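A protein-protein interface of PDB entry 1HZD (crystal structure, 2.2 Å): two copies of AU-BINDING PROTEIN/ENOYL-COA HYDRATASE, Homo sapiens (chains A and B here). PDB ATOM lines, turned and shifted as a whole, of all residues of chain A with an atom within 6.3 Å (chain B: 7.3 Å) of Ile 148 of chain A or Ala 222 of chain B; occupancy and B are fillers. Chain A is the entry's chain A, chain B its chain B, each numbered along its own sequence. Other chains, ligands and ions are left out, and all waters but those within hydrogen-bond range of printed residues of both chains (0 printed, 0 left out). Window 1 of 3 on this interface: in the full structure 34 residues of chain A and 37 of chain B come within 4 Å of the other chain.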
ATOM      1  N   GLU A 122      34.584 -14.837 -24.602  1.00  0.00           N
ATOM      2  CA  GLU A 122      34.085 -13.852 -25.561  1.00  0.00           C
ATOM      3  C   GLU A 122      34.645 -14.123 -26.947  1.00  0.00           C
ATOM      4  O   GLU A 122      33.978 -13.903 -27.959  1.00  0.00           O
ATOM      5  CB  GLU A 122      34.441 -12.436 -25.105  1.00  0.00           C
ATOM      6  CG  GLU A 122      33.567 -11.934 -23.965  1.00  0.00           C
ATOM      7  CD  GLU A 122      34.098 -10.663 -23.349  1.00  0.00           C
ATOM      8  OE1 GLU A 122      33.283  -9.776 -23.020  1.00  0.00           O
ATOM      9  OE2 GLU A 122      35.335 -10.558 -23.186  1.00  0.00           O
ATOM     10  N   GLU A 142      33.592 -10.821 -14.722  1.00  0.00           N
ATOM     11  CA  GLU A 142      33.875  -9.399 -14.590  1.00  0.00           C
ATOM     12  C   GLU A 142      33.197  -8.674 -13.446  1.00  0.00           C
ATOM     13  O   GLU A 142      33.829  -7.859 -12.782  1.00  0.00           O
ATOM     14  CB  GLU A 142      33.559  -8.651 -15.895  1.00  0.00           C
ATOM     15  CG  GLU A 142      34.580  -8.858 -17.022  1.00  0.00           C
ATOM     16  CD  GLU A 142      34.493 -10.243 -17.648  1.00  0.00           C
ATOM     17  OE1 GLU A 142      33.562 -11.006 -17.287  1.00  0.00           O
ATOM     18  OE2 GLU A 142      35.348 -10.562 -18.506  1.00  0.00           O
ATOM     19  N   THR A 143      31.923  -8.949 -13.199  1.00  0.00           N
ATOM     20  CA  THR A 143      31.239  -8.243 -12.129  1.00  0.00           C
ATOM     21  C   THR A 143      31.888  -8.399 -10.754  1.00  0.00           C
ATOM     22  O   THR A 143      31.795  -7.494  -9.926  1.00  0.00           O
ATOM     23  CB  THR A 143      29.771  -8.646 -12.046  1.00  0.00           C
ATOM     24  OG1 THR A 143      29.675 -10.067 -11.927  1.00  0.00           O
ATOM     25  CG2 THR A 143      29.031  -8.174 -13.301  1.00  0.00           C
ATOM     26  N   ALA A 146      34.174  -5.696 -10.360  1.00  0.00           N
ATOM     27  CA  ALA A 146      33.534  -4.393 -10.520  1.00  0.00           C
ATOM     28  C   ALA A 146      33.657  -3.808 -11.921  1.00  0.00           C
ATOM     29  O   ALA A 146      33.675  -2.594 -12.100  1.00  0.00           O
ATOM     30  CB  ALA A 146      34.064  -3.398  -9.481  1.00  0.00           C
ATOM     31  N   ILE A 147      33.763  -4.681 -12.912  1.00  0.00           N
ATOM     32  CA  ILE A 147      33.809  -4.257 -14.305  1.00  0.00           C
ATOM     33  C   ILE A 147      32.772  -5.136 -14.998  1.00  0.00           C
ATOM     34  O   ILE A 147      32.092  -5.921 -14.346  1.00  0.00           O
ATOM     35  CB  ILE A 147      35.194  -4.485 -14.931  1.00  0.00           C
ATOM     36  CG1 ILE A 147      35.652  -5.920 -14.657  1.00  0.00           C
ATOM     37  CG2 ILE A 147      36.183  -3.455 -14.385  1.00  0.00           C
ATOM     38  CD1 ILE A 147      36.979  -6.264 -15.261  1.00  0.00           C
ATOM     39  N   ILE A 148      32.624  -5.008 -16.309  1.00  0.00           N
ATOM     40  CA  ILE A 148      31.653  -5.839 -17.009  1.00  0.00           C
ATOM     41  C   ILE A 148      32.371  -6.483 -18.167  1.00  0.00           C
ATOM     42  O   ILE A 148      33.467  -6.064 -18.521  1.00  0.00           O
ATOM     43  CB  ILE A 148      30.477  -5.011 -17.572  1.00  0.00           C
ATOM     44  CG1 ILE A 148      30.986  -4.043 -18.646  1.00  0.00           C
ATOM     45  CG2 ILE A 148      29.793  -4.263 -16.458  1.00  0.00           C
ATOM     46  CD1 ILE A 148      29.868  -3.408 -19.469  1.00  0.00           C
ATOM     47  N   PRO A 149      31.781  -7.532 -18.761  1.00  0.00           N
ATOM     48  CA  PRO A 149      32.462  -8.159 -19.895  1.00  0.00           C
ATOM     49  C   PRO A 149      32.725  -7.054 -20.916  1.00  0.00           C
ATOM     50  O   PRO A 149      31.802  -6.327 -21.288  1.00  0.00           O
ATOM     51  CB  PRO A 149      31.433  -9.174 -20.391  1.00  0.00           C
ATOM     52  CG  PRO A 149      30.761  -9.598 -19.107  1.00  0.00           C
ATOM     53  CD  PRO A 149      30.558  -8.271 -18.400  1.00  0.00           C
ATOM     54  N   GLY A 150      33.970  -6.921 -21.363  1.00  0.00           N
ATOM     55  CA  GLY A 150      34.283  -5.870 -22.317  1.00  0.00           C
ATOM     56  C   GLY A 150      34.717  -6.323 -23.699  1.00  0.00           C
ATOM     57  O   GLY A 150      35.190  -5.512 -24.494  1.00  0.00           O
ATOM     58  N   GLY A 151      34.550  -7.607 -23.994  1.00  0.00           N
ATOM     59  CA  GLY A 151      34.948  -8.105 -25.298  1.00  0.00           C
ATOM     60  C   GLY A 151      33.780  -8.590 -26.137  1.00  0.00           C
ATOM     61  O   GLY A 151      33.935  -9.523 -26.920  1.00  0.00           O
ATOM     62  N   THR A 154      28.570  -8.934 -23.381  1.00  0.00           N
ATOM     63  CA  THR A 154      27.236  -8.486 -22.973  1.00  0.00           C
ATOM     64  C   THR A 154      26.266  -8.544 -24.132  1.00  0.00           C
ATOM     65  O   THR A 154      25.056  -8.454 -23.943  1.00  0.00           O
ATOM     66  CB  THR A 154      27.231  -7.035 -22.447  1.00  0.00           C
ATOM     67  OG1 THR A 154      27.592  -6.142 -23.511  1.00  0.00           O
ATOM     68  CG2 THR A 154      28.204  -6.886 -21.265  1.00  0.00           C
ATOM     69  N   ILE A 170      26.143 -13.445 -15.831  1.00  0.00           N
ATOM     70  CA  ILE A 170      26.939 -12.239 -15.651  1.00  0.00           C
ATOM     71  C   ILE A 170      26.764 -11.632 -14.254  1.00  0.00           C
ATOM     72  O   ILE A 170      27.735 -11.157 -13.658  1.00  0.00           O
ATOM     73  CB  ILE A 170      26.610 -11.210 -16.767  1.00  0.00           C
ATOM     74  CG1 ILE A 170      27.172 -11.732 -18.100  1.00  0.00           C
ATOM     75  CG2 ILE A 170      27.207  -9.847 -16.448  1.00  0.00           C
ATOM     76  CD1 ILE A 170      26.930 -10.815 -19.295  1.00  0.00           C
ATOM     77  N   PHE A 171      25.539 -11.678 -13.727  1.00  0.00           N
ATOM     78  CA  PHE A 171      25.227 -11.139 -12.399  1.00  0.00           C
ATOM     79  C   PHE A 171      25.878 -11.932 -11.257  1.00  0.00           C
ATOM     80  O   PHE A 171      26.345 -11.359 -10.266  1.00  0.00           O
ATOM     81  CB  PHE A 171      23.711 -11.136 -12.171  1.00  0.00           C
ATOM     82  CG  PHE A 171      22.967 -10.086 -12.958  1.00  0.00           C
ATOM     83  CD1 PHE A 171      21.577 -10.153 -13.078  1.00  0.00           C
ATOM     84  CD2 PHE A 171      23.637  -9.020 -13.542  1.00  0.00           C
ATOM     85  CE1 PHE A 171      20.873  -9.176 -13.764  1.00  0.00           C
ATOM     86  CE2 PHE A 171      22.936  -8.030 -14.234  1.00  0.00           C
ATOM     87  CZ  PHE A 171      21.548  -8.112 -14.343  1.00  0.00           C
ATOM     88  N   PRO B 105      16.996  -0.515 -12.181  1.00  0.00           N
ATOM     89  CA  PRO B 105      18.464  -0.503 -12.262  1.00  0.00           C
ATOM     90  C   PRO B 105      19.234  -1.751 -11.851  1.00  0.00           C
ATOM     91  O   PRO B 105      20.289  -2.046 -12.417  1.00  0.00           O
ATOM     92  CB  PRO B 105      18.860   0.700 -11.391  1.00  0.00           C
ATOM     93  CG  PRO B 105      17.588   1.498 -11.258  1.00  0.00           C
ATOM     94  CD  PRO B 105      16.531   0.447 -11.172  1.00  0.00           C
ATOM     95  N   GLY B 215      30.398  -5.770  -7.818  1.00  0.00           N
ATOM     96  CA  GLY B 215      30.465  -4.316  -7.853  1.00  0.00           C
ATOM     97  C   GLY B 215      29.142  -3.692  -8.249  1.00  0.00           C
ATOM     98  O   GLY B 215      28.697  -3.870  -9.379  1.00  0.00           O
ATOM     99  N   PRO B 216      28.497  -2.933  -7.345  1.00  0.00           N
ATOM    100  CA  PRO B 216      27.205  -2.281  -7.601  1.00  0.00           C
ATOM    101  C   PRO B 216      27.106  -1.505  -8.910  1.00  0.00           C
ATOM    102  O   PRO B 216      26.100  -1.603  -9.615  1.00  0.00           O
ATOM    103  CB  PRO B 216      27.027  -1.382  -6.380  1.00  0.00           C
ATOM    104  CG  PRO B 216      27.713  -2.177  -5.296  1.00  0.00           C
ATOM    105  CD  PRO B 216      28.980  -2.606  -5.992  1.00  0.00           C
ATOM    106  N   VAL B 217      28.146  -0.746  -9.233  1.00  0.00           N
ATOM    107  CA  VAL B 217      28.169   0.049 -10.454  1.00  0.00           C
ATOM    108  C   VAL B 217      28.221  -0.827 -11.701  1.00  0.00           C
ATOM    109  O   VAL B 217      27.475  -0.597 -12.659  1.00  0.00           O
ATOM    110  CB  VAL B 217      29.372   1.006 -10.484  1.00  0.00           C
ATOM    111  CG1 VAL B 217      29.369   1.798 -11.790  1.00  0.00           C
ATOM    112  CG2 VAL B 217      29.313   1.956  -9.286  1.00  0.00           C
ATOM    113  N   ALA B 218      29.094  -1.831 -11.694  1.00  0.00           N
ATOM    114  CA  ALA B 218      29.215  -2.724 -12.840  1.00  0.00           C
ATOM    115  C   ALA B 218      27.933  -3.539 -13.086  1.00  0.00           C
ATOM    116  O   ALA B 218      27.533  -3.747 -14.240  1.00  0.00           O
ATOM    117  CB  ALA B 218      30.409  -3.653 -12.654  1.00  0.00           C
ATOM    118  N   MET B 219      27.293  -4.001 -12.011  1.00  0.00           N
ATOM    119  CA  MET B 219      26.055  -4.776 -12.139  1.00  0.00           C
ATOM    120  C   MET B 219      24.984  -3.941 -12.858  1.00  0.00           C
ATOM    121  O   MET B 219      24.262  -4.443 -13.720  1.00  0.00           O
ATOM    122  CB  MET B 219      25.534  -5.186 -10.756  1.00  0.00           C
ATOM    123  CG  MET B 219      26.390  -6.239 -10.029  1.00  0.00           C
ATOM    124  SD  MET B 219      26.436  -7.868 -10.837  1.00  0.00           S
ATOM    125  CE  MET B 219      25.077  -8.665 -10.008  1.00  0.00           C
ATOM    126  N   ARG B 220      24.894  -2.664 -12.494  1.00  0.00           N
ATOM    127  CA  ARG B 220      23.920  -1.763 -13.091  1.00  0.00           C
ATOM    128  C   ARG B 220      24.175  -1.500 -14.574  1.00  0.00           C
ATOM    129  O   ARG B 220      23.259  -1.620 -15.389  1.00  0.00           O
ATOM    130  CB  ARG B 220      23.877  -0.438 -12.314  1.00  0.00           C
ATOM    131  CG  ARG B 220      23.422  -0.606 -10.861  1.00  0.00           C
ATOM    132  CD  ARG B 220      22.955   0.709 -10.259  1.00  0.00           C
ATOM    133  NE  ARG B 220      22.240   0.511  -8.999  1.00  0.00           N
ATOM    134  CZ  ARG B 220      21.327   1.353  -8.522  1.00  0.00           C
ATOM    135  NH1 ARG B 220      21.021   2.450  -9.202  1.00  0.00           N
ATOM    136  NH2 ARG B 220      20.716   1.096  -7.372  1.00  0.00           N
ATOM    137  N   VAL B 221      25.409  -1.165 -14.940  1.00  0.00           N
ATOM    138  CA  VAL B 221      25.678  -0.898 -16.347  1.00  0.00           C
ATOM    139  C   VAL B 221      25.701  -2.177 -17.166  1.00  0.00           C
ATOM    140  O   VAL B 221      25.528  -2.142 -18.393  1.00  0.00           O
ATOM    141  CB  VAL B 221      26.992  -0.103 -16.555  1.00  0.00           C
ATOM    142  CG1 VAL B 221      26.964   1.160 -15.700  1.00  0.00           C
ATOM    143  CG2 VAL B 221      28.198  -0.966 -16.244  1.00  0.00           C
ATOM    144  N   ALA B 222      25.915  -3.305 -16.492  1.00  0.00           N
ATOM    145  CA  ALA B 222      25.917  -4.600 -17.158  1.00  0.00           C
ATOM    146  C   ALA B 222      24.476  -4.842 -17.604  1.00  0.00           C
ATOM    147  O   ALA B 222      24.223  -5.293 -18.722  1.00  0.00           O
ATOM    148  CB  ALA B 222      26.351  -5.710 -16.190  1.00  0.00           C
ATOM    149  N   LYS B 223      23.539  -4.538 -16.711  1.00  0.00           N
ATOM    150  CA  LYS B 223      22.127  -4.726 -17.005  1.00  0.00           C
ATOM    151  C   LYS B 223      21.715  -3.848 -18.183  1.00  0.00           C
ATOM    152  O   LYS B 223      20.974  -4.304 -19.057  1.00  0.00           O
ATOM    153  CB  LYS B 223      21.255  -4.402 -15.788  1.00  0.00           C
ATOM    154  CG  LYS B 223      19.754  -4.528 -16.083  1.00  0.00           C
ATOM    155  CD  LYS B 223      18.903  -4.713 -14.836  1.00  0.00           C
ATOM    156  CE  LYS B 223      17.436  -4.838 -15.227  1.00  0.00           C
ATOM    157  NZ  LYS B 223      16.569  -5.276 -14.103  1.00  0.00           N
ATOM    158  N   LEU B 224      22.200  -2.603 -18.196  1.00  0.00           N
ATOM    159  CA  LEU B 224      21.893  -1.664 -19.266  1.00  0.00           C
ATOM    160  C   LEU B 224      22.444  -2.121 -20.618  1.00  0.00           C
ATOM    161  O   LEU B 224      21.772  -1.995 -21.644  1.00  0.00           O
ATOM    162  CB  LEU B 224      22.441  -0.267 -18.937  1.00  0.00           C
ATOM    163  CG  LEU B 224      21.819   0.467 -17.738  1.00  0.00           C
ATOM    164  CD1 LEU B 224      22.558   1.786 -17.486  1.00  0.00           C
ATOM    165  CD2 LEU B 224      20.341   0.740 -18.004  1.00  0.00           C
ATOM    166  N   ALA B 225      23.661  -2.652 -20.628  1.00  0.00           N
ATOM    167  CA  ALA B 225      24.256  -3.101 -21.882  1.00  0.00           C
ATOM    168  C   ALA B 225      23.474  -4.289 -22.440  1.00  0.00           C
ATOM    169  O   ALA B 225      23.295  -4.415 -23.654  1.00  0.00           O
ATOM    170  CB  ALA B 225      25.745  -3.481 -21.678  1.00  0.00           C
ATOM    171  N   ILE B 226      23.006  -5.158 -21.556  1.00  0.00           N
ATOM    172  CA  ILE B 226      22.254  -6.331 -21.995  1.00  0.00           C
ATOM    173  C   ILE B 226      20.849  -5.943 -22.465  1.00  0.00           C
ATOM    174  O   ILE B 226      20.455  -6.244 -23.601  1.00  0.00           O
ATOM    175  CB  ILE B 226      22.193  -7.384 -20.862  1.00  0.00           C
ATOM    176  CG1 ILE B 226      23.612  -7.911 -20.596  1.00  0.00           C
ATOM    177  CG2 ILE B 226      21.249  -8.539 -21.231  1.00  0.00           C
ATOM    178  CD1 ILE B 226      23.715  -8.892 -19.405  1.00  0.00           C
ATOM    179  N   ASN B 227      20.094  -5.260 -21.612  1.00  0.00           N
ATOM    180  CA  ASN B 227      18.740  -4.858 -21.996  1.00  0.00           C
ATOM    181  C   ASN B 227      18.729  -4.008 -23.263  1.00  0.00           C
ATOM    182  O   ASN B 227      17.950  -4.267 -24.179  1.00  0.00           O
ATOM    183  CB  ASN B 227      18.051  -4.079 -20.868  1.00  0.00           C
ATOM    184  CG  ASN B 227      17.359  -4.984 -19.869  1.00  0.00           C
ATOM    185  OD1 ASN B 227      17.308  -6.204 -20.048  1.00  0.00           O
ATOM    186  ND2 ASN B 227      16.805  -4.391 -18.816  1.00  0.00           N
ATOM    187  N   GLN B 228      19.595  -3.003 -23.320  1.00  0.00           N
ATOM    188  CA  GLN B 228      19.655  -2.117 -24.478  1.00  0.00           C
ATOM    189  C   GLN B 228      20.241  -2.776 -25.724  1.00  0.00           C
ATOM    190  O   GLN B 228      19.664  -2.699 -26.808  1.00  0.00           O
ATOM    191  CB  GLN B 228      20.482  -0.875 -24.149  1.00  0.00           C
ATOM    192  CG  GLN B 228      19.929  -0.011 -23.037  1.00  0.00           C
ATOM    193  CD  GLN B 228      20.944   1.035 -22.575  1.00  0.00           C
ATOM    194  OE1 GLN B 228      21.604   1.681 -23.398  1.00  0.00           O
ATOM    195  NE2 GLN B 228      21.066   1.210 -21.258  1.00  0.00           N
ATOM    196  N   ILE B 240      27.460   0.202 -27.231  1.00  0.00           N
ATOM    197  CA  ILE B 240      26.807   0.431 -25.957  1.00  0.00           C
ATOM    198  C   ILE B 240      27.625  -0.254 -24.859  1.00  0.00           C
ATOM    199  O   ILE B 240      27.842   0.316 -23.794  1.00  0.00           O
ATOM    200  CB  ILE B 240      25.359  -0.097 -25.963  1.00  0.00           C
ATOM    201  CG1 ILE B 240      24.516   0.732 -26.946  1.00  0.00           C
ATOM    202  CG2 ILE B 240      24.781  -0.028 -24.554  1.00  0.00           C
ATOM    203  CD1 ILE B 240      23.062   0.290 -27.073  1.00  0.00           C
ATOM    204  N   GLU B 241      28.093  -1.471 -25.132  1.00  0.00           N
ATOM    205  CA  GLU B 241      28.904  -2.200 -24.154  1.00  0.00           C
ATOM    206  C   GLU B 241      30.137  -1.360 -23.826  1.00  0.00           C
ATOM    207  O   GLU B 241      30.592  -1.335 -22.683  1.00  0.00           O
ATOM    208  CB  GLU B 241      29.347  -3.561 -24.709  1.00  0.00           C
ATOM    209  CG  GLU B 241      30.320  -4.297 -23.787  1.00  0.00           C
ATOM    210  CD  GLU B 241      30.798  -5.613 -24.364  1.00  0.00           C
ATOM    211  OE1 GLU B 241      29.979  -6.558 -24.447  1.00  0.00           O
ATOM    212  OE2 GLU B 241      31.988  -5.696 -24.739  1.00  0.00           O
ATOM    213  N   GLU B 242      30.673  -0.672 -24.835  1.00  0.00           N
ATOM    214  CA  GLU B 242      31.845   0.176 -24.627  1.00  0.00           C
ATOM    215  C   GLU B 242      31.516   1.362 -23.721  1.00  0.00           C
ATOM    216  O   GLU B 242      32.274   1.682 -22.810  1.00  0.00           O
ATOM    217  CB  GLU B 242      32.383   0.683 -25.970  1.00  0.00           C
ATOM    218  CG  GLU B 242      33.604   1.599 -25.848  1.00  0.00           C
ATOM    219  CD  GLU B 242      34.115   2.084 -27.198  1.00  0.00           C
ATOM    220  OE1 GLU B 242      34.795   1.312 -27.906  1.00  0.00           O
ATOM    221  OE2 GLU B 242      33.823   3.243 -27.556  1.00  0.00           O
ATOM    222  N   ALA B 243      30.378   2.003 -23.952  1.00  0.00           N
ATOM    223  CA  ALA B 243      29.999   3.152 -23.139  1.00  0.00           C
ATOM    224  C   ALA B 243      29.662   2.745 -21.710  1.00  0.00           C
ATOM    225  O   ALA B 243      29.844   3.529 -20.774  1.00  0.00           O
ATOM    226  CB  ALA B 243      28.830   3.882 -23.771  1.00  0.00           C
ATOM    227  N   CYS B 244      29.177   1.518 -21.538  1.00  0.00           N
ATOM    228  CA  CYS B 244      28.842   1.024 -20.208  1.00  0.00           C
ATOM    229  C   CYS B 244      30.127   0.642 -19.462  1.00  0.00           C
ATOM    230  O   CYS B 244      30.288   0.973 -18.286  1.00  0.00           O
ATOM    231  CB  CYS B 244      27.889  -0.177 -20.316  1.00  0.00           C
ATOM    232  SG  CYS B 244      26.174   0.281 -20.829  1.00  0.00           S
ATOM    233  N   TYR B 245      31.042  -0.039 -20.151  1.00  0.00           N
ATOM    234  CA  TYR B 245      32.309  -0.430 -19.544  1.00  0.00           C
ATOM    235  C   TYR B 245      33.029   0.827 -19.069  1.00  0.00           C
ATOM    236  O   TYR B 245      33.504   0.888 -17.935  1.00  0.00           O
ATOM    237  CB  TYR B 245      33.211  -1.161 -20.546  1.00  0.00           C
ATOM    238  CG  TYR B 245      34.439  -1.788 -19.902  1.00  0.00           C
ATOM    239  CD1 TYR B 245      34.390  -3.070 -19.344  1.00  0.00           C
ATOM    240  CD2 TYR B 245      35.633  -1.078 -19.805  1.00  0.00           C
ATOM    241  CE1 TYR B 245      35.505  -3.626 -18.697  1.00  0.00           C
ATOM    242  CE2 TYR B 245      36.748  -1.618 -19.167  1.00  0.00           C
ATOM    243  CZ  TYR B 245      36.681  -2.886 -18.613  1.00  0.00           C
ATOM    244  OH  TYR B 245      37.792  -3.386 -17.972  1.00  0.00           O
ATOM    245  N   ALA B 246      33.091   1.833 -19.945  1.00  0.00           N
ATOM    246  CA  ALA B 246      33.765   3.091 -19.638  1.00  0.00           C
ATOM    247  C   ALA B 246      33.335   3.692 -18.298  1.00  0.00           C
ATOM    248  O   ALA B 246      34.125   4.348 -17.620  1.00  0.00           O
ATOM    249  CB  ALA B 246      33.540   4.121 -20.786  1.00  0.00           C
ATOM    250  N   THR B 248      32.717   2.085 -15.587  1.00  0.00           N
ATOM    251  CA  THR B 248      33.266   1.376 -14.430  1.00  0.00           C
ATOM    252  C   THR B 248      34.743   1.699 -14.205  1.00  0.00           C
ATOM    253  O   THR B 248      35.254   1.520 -13.107  1.00  0.00           O
ATOM    254  CB  THR B 248      33.166  -0.168 -14.556  1.00  0.00           C
ATOM    255  OG1 THR B 248      34.069  -0.628 -15.576  1.00  0.00           O
ATOM    256  CG2 THR B 248      31.746  -0.598 -14.871  1.00  0.00           C
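The side-chain hydroxyl (OG1) of Thr 154 of chain A lies within hydrogen-bond range of the side-chain carboxylate (OE1) of Glu 241 of chain B.
The backbone carbonyl oxygen (O) of Thr 143 of chain A lies within hydrogen-bond range of the backbone NH (N) of Gly 215 of chain B, at 3.1 Å.
N of Gly 151 of chain A is in hydrogen-bond range of OE2 of Glu 241 of chain B (3.3 Å).
The side-chain carboxylate of Glu 241 of chain B lies close to the backbone carbonyl oxygen of Gly 150 of chain A (3.2 Å).
The backbone carbonyl oxygen (O) of Phe 171 of chain A lies close to the side-chain sulfur (SD) of Met 219 of chain B, 3.5 Å away.
SG of Cys 244 of chain B is in hydrogen-bond range of O of Ile 240 of chain B, 3.4 Å away.
The backbone carbonyl oxygen (O) of Tyr 245 of chain B lies within hydrogen-bond range of the side-chain hydroxyl (OG1) of Thr 248 of chain B, 2.9 Å away.
The side-chain hydroxyl of Thr 143 of chain A sits at hydrogen-bond distance from the backbone carbonyl oxygen of Ile 170 of chain A (2.8 Å).
The side-chain carboxylate (OE1) of Glu 122 of chain A lies within hydrogen-bond range of the backbone NH (N) of Gly 150 of chain A, 3.4 Å away.
SG of Cys 244 of chain B lies within hydrogen-bond range of O of Val 221 of chain B (3.5 Å).
The side-chain carboxylate (OE1) of Glu 122 of chain A is in hydrogen-bond range of the backbone NH (N) of Gly 151 of chain A (2.7 Å).
Among the printed residues, merely in contact across the chains: Thr 143 of chain A with Met 219 of chain B, Ala 146 of chain A with Ala 218 of chain B, Ala 146 of chain A with Thr 248 of chain B, Ile 147 of chain A with Ala 218 of chain B, Ile 147 of chain A with Tyr 245 of chain B, Ile 147 of chain A with Thr 248 of chain B, Ile 148 of chain A with Ala 218 of chain B, Ile 148 of chain A with Val 221 of chain B, Ile 148 of chain A with Ala 222 of chain B, Ile 148 of chain A with Glu 241 of chain B, Ile 148 of chain A with Cys 244 of chain B, Ile 148 of chain A with Tyr 245 of chain B, Pro 149 of chain A with Glu 241 of chain B, Thr 154 of chain A with Ala 225 of chain B, Thr 154 of chain A with Ile 226 of chain B, Ile 170 of chain A with Ile 226 of chain B and Phe 171 of chain A with Lys 223 of chain B.
Of the printed residues of chain B, Ile 147 of chain A touches Ala 218 (3.3 Å), Tyr 245 (3.9 Å) and Thr 248 (3.7 Å).
Of the printed residues of chain B, Ile 148 of chain A touches Ala 218, Val 221, Ala 222, Glu 241, Cys 244 and Tyr 245.
Printed residues of chain B within 4 Å of Gly 150 of chain A: Glu 241.
Printed residues of chain A within 4 Å of Lys 223 of chain B: Phe 171.
Of the printed residues of chain A, Ala 225 of chain B touches Thr 154 (3.7 Å).
Asn 227 of chain B touches none of the printed residues of chain A.
Ala 246 of chain B touches none of the printed residues of chain A.
The nearest printed residue of chain A that does not touch Val 221 of chain B is Thr 154 of chain A (6.2 Å).
Hydrophobic or aromatic side chains of chain A that line the printed part of chain B: Ile 147, Ile 148, Ile 170 and Phe 171.
Of the 23 printed residues of chain B, 12 touch a printed residue of chain A.
Hydrophobic or aromatic side chains of chain B within 4 Å of the printed part of chain A: Ala 218, Met 219, Val 221, Ala 222, Ala 225, Ile 226 and Tyr 245.
Among the printed residues, no Asp or Glu carboxylate lies within 4 Å of a Lys or Arg side-chain nitrogen of the other chain.
No position is printed for both chains.
Of the 22 pairs that touch across the chains among the printed residues, none has its exchanged pair printed and touching as well.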
